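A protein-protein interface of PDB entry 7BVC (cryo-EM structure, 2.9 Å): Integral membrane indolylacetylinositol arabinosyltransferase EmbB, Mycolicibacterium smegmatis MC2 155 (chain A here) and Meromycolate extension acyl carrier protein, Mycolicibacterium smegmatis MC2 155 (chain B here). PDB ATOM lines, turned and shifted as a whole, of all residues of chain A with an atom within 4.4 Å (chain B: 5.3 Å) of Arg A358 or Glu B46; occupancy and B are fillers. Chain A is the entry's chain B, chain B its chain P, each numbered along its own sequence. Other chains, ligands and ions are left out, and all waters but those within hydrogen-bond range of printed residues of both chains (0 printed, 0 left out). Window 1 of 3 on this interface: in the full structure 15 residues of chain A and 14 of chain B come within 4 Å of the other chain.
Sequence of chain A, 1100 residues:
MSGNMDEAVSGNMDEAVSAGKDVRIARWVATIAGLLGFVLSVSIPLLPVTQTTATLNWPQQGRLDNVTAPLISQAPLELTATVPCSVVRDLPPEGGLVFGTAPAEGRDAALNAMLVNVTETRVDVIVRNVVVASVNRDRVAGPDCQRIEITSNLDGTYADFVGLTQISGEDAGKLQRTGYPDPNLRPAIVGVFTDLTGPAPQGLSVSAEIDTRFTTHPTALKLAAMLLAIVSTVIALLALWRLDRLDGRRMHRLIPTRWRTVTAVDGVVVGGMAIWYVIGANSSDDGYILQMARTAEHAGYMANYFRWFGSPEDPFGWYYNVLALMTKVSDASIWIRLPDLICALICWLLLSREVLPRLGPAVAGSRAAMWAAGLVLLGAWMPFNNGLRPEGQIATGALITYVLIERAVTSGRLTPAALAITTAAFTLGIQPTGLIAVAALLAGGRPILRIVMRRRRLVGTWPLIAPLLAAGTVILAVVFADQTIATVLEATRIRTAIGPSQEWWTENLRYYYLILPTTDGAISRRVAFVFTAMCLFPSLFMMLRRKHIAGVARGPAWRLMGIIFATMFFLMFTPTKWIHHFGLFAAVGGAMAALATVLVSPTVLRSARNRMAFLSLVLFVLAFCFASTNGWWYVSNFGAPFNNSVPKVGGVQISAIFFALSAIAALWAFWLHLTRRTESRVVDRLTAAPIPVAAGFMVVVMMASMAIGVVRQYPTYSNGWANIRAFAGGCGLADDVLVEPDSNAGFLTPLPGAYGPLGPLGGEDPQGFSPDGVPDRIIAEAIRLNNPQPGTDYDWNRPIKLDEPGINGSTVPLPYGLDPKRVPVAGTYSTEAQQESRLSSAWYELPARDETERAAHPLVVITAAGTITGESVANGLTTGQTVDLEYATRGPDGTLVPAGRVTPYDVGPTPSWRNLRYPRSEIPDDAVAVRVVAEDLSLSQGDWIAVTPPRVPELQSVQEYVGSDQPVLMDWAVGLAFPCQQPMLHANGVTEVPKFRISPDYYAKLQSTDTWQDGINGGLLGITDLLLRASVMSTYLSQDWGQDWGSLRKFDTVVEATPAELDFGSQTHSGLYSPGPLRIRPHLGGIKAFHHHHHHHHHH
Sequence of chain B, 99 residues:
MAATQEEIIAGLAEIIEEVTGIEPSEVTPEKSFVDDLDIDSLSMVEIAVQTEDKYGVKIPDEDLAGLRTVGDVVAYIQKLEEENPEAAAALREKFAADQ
OE1 of Glu B46 lies within hydrogen-bond range of OG1 of Thr A410, 3.3 Å away.
The side-chain carboxylate of Glu B46 is in salt-bridge range of the guanidinium group of Arg A358 (3.2 Å).
Among the printed residues, pairs that only touch across the chains: Thr A410 with Leu B42 (3.4 Å) and Ala A553 with Val B19 (3.6 Å).
Arg A358 touches just one residue of chain B: Glu B46 (3.2 Å).
Of chain A, only Arg A358 and Thr A410 come within 4 Å of Glu B46.
Printed residues of chain A within 4 Å of Leu B42: Thr A410 (3.4 Å).
Printed residues of chain B within 4 Å of Ala A553: Val B19.
Of the printed residues of chain B, Thr A410 touches Leu B42 (3.4 Å) and Glu B46 (3.3 Å).
Leu A359 touches none of the printed residues of chain B.
Pro A357 touches none of the printed residues of chain B.
The nearest printed residue of chain A that does not touch Glu B46 is Val A409 (4.8 Å).
Printed residues of chain B that touch a printed residue of chain A: Val B19, Leu B42 and Glu B46.
Of the 12 printed residues of chain A, 3 touch a printed residue of chain B.
Hydrophobic or aromatic side chains of chain A within 4 Å of the printed part of chain B: Ala A553.
Among the printed residues, Asp or Glu carboxylates within 4 Å of a Lys or Arg side-chain nitrogen of the other chain: Arg A358 with Glu B46 (3.2 Å).
The side-chain carboxylate (OE1) of Glu A406 lies within salt-bridge range of the guanidinium group (NE) of Arg A358, 3.0 Å away.
The guanidinium group (NH2) of Arg A358 is in hydrogen-bond range of the side-chain hydroxyl (OG1) of Thr A410.
O of Glu A406 sits at hydrogen-bond distance from OG1 of Thr A410, 3.1 Å away.
The backbone carbonyl oxygen of Leu A359 is in hydrogen-bond range of the backbone NH of Ala A553 (3.3 Å).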
ATOM      1  N   GLU A 354     -31.445  31.004  16.514  1.00  0.00           N
ATOM      2  CA  GLU A 354     -32.006  29.681  16.757  1.00  0.00           C
ATOM      3  C   GLU A 354     -32.294  28.913  15.479  1.00  0.00           C
ATOM      4  O   GLU A 354     -32.141  27.691  15.456  1.00  0.00           O
ATOM      5  CB  GLU A 354     -33.293  29.797  17.589  1.00  0.00           C
ATOM      6  CG  GLU A 354     -33.090  30.359  18.983  1.00  0.00           C
ATOM      7  CD  GLU A 354     -32.287  29.432  19.873  1.00  0.00           C
ATOM      8  OE1 GLU A 354     -32.453  28.201  19.753  1.00  0.00           O
ATOM      9  OE2 GLU A 354     -31.489  29.933  20.690  1.00  0.00           O
ATOM     10  N   VAL A 355     -32.711  29.595  14.415  1.00  0.00           N
ATOM     11  CA  VAL A 355     -33.148  28.915  13.202  1.00  0.00           C
ATOM     12  C   VAL A 355     -32.000  28.727  12.219  1.00  0.00           C
ATOM     13  O   VAL A 355     -31.897  27.683  11.571  1.00  0.00           O
ATOM     14  CB  VAL A 355     -34.316  29.694  12.562  1.00  0.00           C
ATOM     15  CG1 VAL A 355     -34.737  29.051  11.255  1.00  0.00           C
ATOM     16  CG2 VAL A 355     -35.489  29.768  13.522  1.00  0.00           C
ATOM     17  N   LEU A 356     -31.115  29.711  12.097  1.00  0.00           N
ATOM     18  CA  LEU A 356     -30.013  29.606  11.149  1.00  0.00           C
ATOM     19  C   LEU A 356     -28.922  28.658  11.644  1.00  0.00           C
ATOM     20  O   LEU A 356     -28.419  27.854  10.850  1.00  0.00           O
ATOM     21  CB  LEU A 356     -29.426  30.986  10.843  1.00  0.00           C
ATOM     22  CG  LEU A 356     -30.321  31.951  10.064  1.00  0.00           C
ATOM     23  CD1 LEU A 356     -29.504  33.109   9.527  1.00  0.00           C
ATOM     24  CD2 LEU A 356     -31.043  31.237   8.939  1.00  0.00           C
ATOM     25  N   PRO A 357     -28.510  28.707  12.920  1.00  0.00           N
ATOM     26  CA  PRO A 357     -27.551  27.699  13.398  1.00  0.00           C
ATOM     27  C   PRO A 357     -28.105  26.288  13.412  1.00  0.00           C
ATOM     28  O   PRO A 357     -27.321  25.335  13.486  1.00  0.00           O
ATOM     29  CB  PRO A 357     -27.213  28.177  14.816  1.00  0.00           C
ATOM     30  CG  PRO A 357     -27.504  29.622  14.798  1.00  0.00           C
ATOM     31  CD  PRO A 357     -28.712  29.759  13.932  1.00  0.00           C
ATOM     32  N   ARG A 358     -29.426  26.118  13.348  1.00  0.00           N
ATOM     33  CA  ARG A 358     -30.013  24.786  13.343  1.00  0.00           C
ATOM     34  C   ARG A 358     -29.933  24.131  11.970  1.00  0.00           C
ATOM     35  O   ARG A 358     -29.929  22.900  11.875  1.00  0.00           O
ATOM     36  CB  ARG A 358     -31.468  24.858  13.813  1.00  0.00           C
ATOM     37  CG  ARG A 358     -32.140  23.513  14.007  1.00  0.00           C
ATOM     38  CD  ARG A 358     -31.655  22.829  15.269  1.00  0.00           C
ATOM     39  NE  ARG A 358     -32.434  21.635  15.573  1.00  0.00           N
ATOM     40  CZ  ARG A 358     -31.978  20.393  15.448  1.00  0.00           C
ATOM     41  NH1 ARG A 358     -30.741  20.179  15.022  1.00  0.00           N
ATOM     42  NH2 ARG A 358     -32.757  19.367  15.750  1.00  0.00           N
ATOM     43  N   LEU A 359     -29.855  24.927  10.906  1.00  0.00           N
ATOM     44  CA  LEU A 359     -29.844  24.408   9.545  1.00  0.00           C
ATOM     45  C   LEU A 359     -28.477  23.897   9.106  1.00  0.00           C
ATOM     46  O   LEU A 359     -28.329  23.508   7.945  1.00  0.00           O
ATOM     47  CB  LEU A 359     -30.324  25.485   8.568  1.00  0.00           C
ATOM     48  CG  LEU A 359     -31.811  25.835   8.613  1.00  0.00           C
ATOM     49  CD1 LEU A 359     -32.075  27.141   7.886  1.00  0.00           C
ATOM     50  CD2 LEU A 359     -32.637  24.718   8.016  1.00  0.00           C
ATOM     51  N   GLY A 360     -27.482  23.888   9.987  1.00  0.00           N
ATOM     52  CA  GLY A 360     -26.190  23.339   9.659  1.00  0.00           C
ATOM     53  C   GLY A 360     -25.062  24.337   9.817  1.00  0.00           C
ATOM     54  O   GLY A 360     -25.282  25.546   9.931  1.00  0.00           O
ATOM     55  N   GLU A 406     -38.258  22.413  17.739  1.00  0.00           N
ATOM     56  CA  GLU A 406     -36.877  22.035  17.463  1.00  0.00           C
ATOM     57  C   GLU A 406     -36.091  21.814  18.749  1.00  0.00           C
ATOM     58  O   GLU A 406     -35.244  20.918  18.805  1.00  0.00           O
ATOM     59  CB  GLU A 406     -36.201  23.093  16.596  1.00  0.00           C
ATOM     60  CG  GLU A 406     -36.762  23.182  15.188  1.00  0.00           C
ATOM     61  CD  GLU A 406     -36.314  22.033  14.308  1.00  0.00           C
ATOM     62  OE1 GLU A 406     -35.327  21.358  14.663  1.00  0.00           O
ATOM     63  OE2 GLU A 406     -36.951  21.807  13.256  1.00  0.00           O
ATOM     64  N   VAL A 409     -37.038  18.386  19.938  1.00  0.00           N
ATOM     65  CA  VAL A 409     -36.359  17.359  19.150  1.00  0.00           C
ATOM     66  C   VAL A 409     -34.894  17.257  19.558  1.00  0.00           C
ATOM     67  O   VAL A 409     -34.334  16.158  19.649  1.00  0.00           O
ATOM     68  CB  VAL A 409     -36.512  17.654  17.646  1.00  0.00           C
ATOM     69  CG1 VAL A 409     -35.606  16.752  16.831  1.00  0.00           C
ATOM     70  CG2 VAL A 409     -37.958  17.487  17.218  1.00  0.00           C
ATOM     71  N   THR A 410     -34.254  18.398  19.818  1.00  0.00           N
ATOM     72  CA  THR A 410     -32.839  18.401  20.174  1.00  0.00           C
ATOM     73  C   THR A 410     -32.610  17.752  21.535  1.00  0.00           C
ATOM     74  O   THR A 410     -31.875  16.768  21.652  1.00  0.00           O
ATOM     75  CB  THR A 410     -32.302  19.833  20.164  1.00  0.00           C
ATOM     76  OG1 THR A 410     -32.216  20.305  18.816  1.00  0.00           O
ATOM     77  CG2 THR A 410     -30.926  19.892  20.805  1.00  0.00           C
ATOM     78  N   ALA A 553     -28.205  20.245   7.306  1.00  0.00           N
ATOM     79  CA  ALA A 553     -28.944  19.163   7.937  1.00  0.00           C
ATOM     80  C   ALA A 553     -30.240  18.926   7.175  1.00  0.00           C
ATOM     81  O   ALA A 553     -30.961  19.875   6.855  1.00  0.00           O
ATOM     82  CB  ALA A 553     -29.235  19.493   9.397  1.00  0.00           C
ATOM     83  N   PRO A 556     -34.021  19.519   9.530  1.00  0.00           N
ATOM     84  CA  PRO A 556     -34.413  20.926   9.705  1.00  0.00           C
ATOM     85  C   PRO A 556     -34.600  21.675   8.399  1.00  0.00           C
ATOM     86  O   PRO A 556     -35.324  22.678   8.381  1.00  0.00           O
ATOM     87  CB  PRO A 556     -33.259  21.514  10.524  1.00  0.00           C
ATOM     88  CG  PRO A 556     -32.667  20.354  11.227  1.00  0.00           C
ATOM     89  CD  PRO A 556     -32.816  19.185  10.308  1.00  0.00           C
ATOM     90  N   VAL B  19     -26.997  14.627  12.580  1.00  0.00           N
ATOM     91  CA  VAL B  19     -27.363  15.794  13.376  1.00  0.00           C
ATOM     92  C   VAL B  19     -27.044  17.079  12.620  1.00  0.00           C
ATOM     93  O   VAL B  19     -27.931  17.895  12.347  1.00  0.00           O
ATOM     94  CB  VAL B  19     -26.660  15.759  14.744  1.00  0.00           C
ATOM     95  CG1 VAL B  19     -26.785  17.102  15.439  1.00  0.00           C
ATOM     96  CG2 VAL B  19     -27.239  14.651  15.603  1.00  0.00           C
ATOM     97  N   SER B  41     -22.327  23.305  21.431  1.00  0.00           N
ATOM     98  CA  SER B  41     -22.677  22.300  22.427  1.00  0.00           C
ATOM     99  C   SER B  41     -24.159  21.953  22.411  1.00  0.00           C
ATOM    100  O   SER B  41     -24.531  20.861  22.857  1.00  0.00           O
ATOM    101  CB  SER B  41     -22.272  22.775  23.815  1.00  0.00           C
ATOM    102  OG  SER B  41     -22.992  23.939  24.154  1.00  0.00           O
ATOM    103  N   LEU B  42     -25.013  22.848  21.912  1.00  0.00           N
ATOM    104  CA  LEU B  42     -26.414  22.495  21.716  1.00  0.00           C
ATOM    105  C   LEU B  42     -26.592  21.402  20.674  1.00  0.00           C
ATOM    106  O   LEU B  42     -27.677  20.818  20.588  1.00  0.00           O
ATOM    107  CB  LEU B  42     -27.224  23.729  21.316  1.00  0.00           C
ATOM    108  CG  LEU B  42     -28.014  24.371  22.457  1.00  0.00           C
ATOM    109  CD1 LEU B  42     -28.676  25.662  22.012  1.00  0.00           C
ATOM    110  CD2 LEU B  42     -29.045  23.394  22.986  1.00  0.00           C
ATOM    111  N   SER B  43     -25.558  21.118  19.884  1.00  0.00           N
ATOM    112  CA  SER B  43     -25.523  19.944  19.024  1.00  0.00           C
ATOM    113  C   SER B  43     -24.797  18.773  19.663  1.00  0.00           C
ATOM    114  O   SER B  43     -25.101  17.619  19.342  1.00  0.00           O
ATOM    115  CB  SER B  43     -24.855  20.279  17.689  1.00  0.00           C
ATOM    116  OG  SER B  43     -25.614  21.221  16.958  1.00  0.00           O
ATOM    117  N   MET B  44     -23.847  19.038  20.562  1.00  0.00           N
ATOM    118  CA  MET B  44     -23.234  17.954  21.318  1.00  0.00           C
ATOM    119  C   MET B  44     -24.252  17.262  22.211  1.00  0.00           C
ATOM    120  O   MET B  44     -24.182  16.043  22.402  1.00  0.00           O
ATOM    121  CB  MET B  44     -22.064  18.484  22.144  1.00  0.00           C
ATOM    122  CG  MET B  44     -20.773  18.640  21.362  1.00  0.00           C
ATOM    123  SD  MET B  44     -20.065  17.058  20.874  1.00  0.00           S
ATOM    124  CE  MET B  44     -19.579  16.406  22.469  1.00  0.00           C
ATOM    125  N   VAL B  45     -25.213  18.014  22.748  1.00  0.00           N
ATOM    126  CA  VAL B  45     -26.284  17.399  23.530  1.00  0.00           C
ATOM    127  C   VAL B  45     -27.118  16.473  22.653  1.00  0.00           C
ATOM    128  O   VAL B  45     -27.481  15.362  23.061  1.00  0.00           O
ATOM    129  CB  VAL B  45     -27.154  18.480  24.195  1.00  0.00           C
ATOM    130  CG1 VAL B  45     -28.290  17.843  24.979  1.00  0.00           C
ATOM    131  CG2 VAL B  45     -26.310  19.357  25.099  1.00  0.00           C
ATOM    132  N   GLU B  46     -27.421  16.904  21.429  1.00  0.00           N
ATOM    133  CA  GLU B  46     -28.195  16.062  20.524  1.00  0.00           C
ATOM    134  C   GLU B  46     -27.407  14.821  20.118  1.00  0.00           C
ATOM    135  O   GLU B  46     -27.977  13.732  19.981  1.00  0.00           O
ATOM    136  CB  GLU B  46     -28.607  16.865  19.293  1.00  0.00           C
ATOM    137  CG  GLU B  46     -29.550  16.133  18.359  1.00  0.00           C
ATOM    138  CD  GLU B  46     -30.170  17.054  17.325  1.00  0.00           C
ATOM    139  OE1 GLU B  46     -29.981  18.282  17.436  1.00  0.00           O
ATOM    140  OE2 GLU B  46     -30.848  16.549  16.404  1.00  0.00           O
ATOM    141  N   ILE B  47     -26.097  14.968  19.921  1.00  0.00           N
ATOM    142  CA  ILE B  47     -25.261  13.815  19.599  1.00  0.00           C
ATOM    143  C   ILE B  47     -25.242  12.833  20.763  1.00  0.00           C
ATOM    144  O   ILE B  47     -25.345  11.618  20.567  1.00  0.00           O
ATOM    145  CB  ILE B  47     -23.841  14.274  19.216  1.00  0.00           C
ATOM    146  CG1 ILE B  47     -23.867  15.056  17.903  1.00  0.00           C
ATOM    147  CG2 ILE B  47     -22.905  13.083  19.102  1.00  0.00           C
ATOM    148  CD1 ILE B  47     -22.541  15.667  17.531  1.00  0.00           C
ATOM    149  N   ALA B  48     -25.140  13.342  21.992  1.00  0.00           N
ATOM    150  CA  ALA B  48     -25.134  12.465  23.158  1.00  0.00           C
ATOM    151  C   ALA B  48     -26.495  11.836  23.420  1.00  0.00           C
ATOM    152  O   ALA B  48     -26.566  10.797  24.083  1.00  0.00           O
ATOM    153  CB  ALA B  48     -24.673  13.234  24.395  1.00  0.00           C
ATOM    154  N   VAL B  49     -27.572  12.446  22.931  1.00  0.00           N
ATOM    155  CA  VAL B  49     -28.890  11.827  23.045  1.00  0.00           C
ATOM    156  C   VAL B  49     -29.056  10.721  22.010  1.00  0.00           C
ATOM    157  O   VAL B  49     -29.469   9.599  22.331  1.00  0.00           O
ATOM    158  CB  VAL B  49     -29.993  12.894  22.916  1.00  0.00           C
ATOM    159  CG1 VAL B  49     -31.340  12.236  22.683  1.00  0.00           C
ATOM    160  CG2 VAL B  49     -30.035  13.761  24.159  1.00  0.00           C
ATOM    161  N   GLN B  50     -28.727  11.017  20.751  1.00  0.00           N
ATOM    162  CA  GLN B  50     -28.836  10.011  19.701  1.00  0.00           C
ATOM    163  C   GLN B  50     -27.828   8.882  19.871  1.00  0.00           C
ATOM    164  O   GLN B  50     -28.026   7.803  19.305  1.00  0.00           O
ATOM    165  CB  GLN B  50     -28.669  10.658  18.328  1.00  0.00           C
ATOM    166  CG  GLN B  50     -29.780  11.624  17.969  1.00  0.00           C
ATOM    167  CD  GLN B  50     -29.857  11.892  16.483  1.00  0.00           C
ATOM    168  OE1 GLN B  50     -29.240  11.188  15.683  1.00  0.00           O
ATOM    169  NE2 GLN B  50     -30.616  12.912  16.102  1.00  0.00           N
ATOM    170  N   THR B  51     -26.752   9.105  20.626  1.00  0.00           N
ATOM    171  CA  THR B  51     -25.846   8.013  20.954  1.00  0.00           C
ATOM    172  C   THR B  51     -26.532   6.995  21.854  1.00  0.00           C
ATOM    173  O   THR B  51     -26.472   5.788  21.605  1.00  0.00           O
ATOM    174  CB  THR B  51     -24.585   8.558  21.627  1.00  0.00           C
ATOM    175  OG1 THR B  51     -23.814   9.298  20.675  1.00  0.00           O
ATOM    176  CG2 THR B  51     -23.744   7.420  22.176  1.00  0.00           C
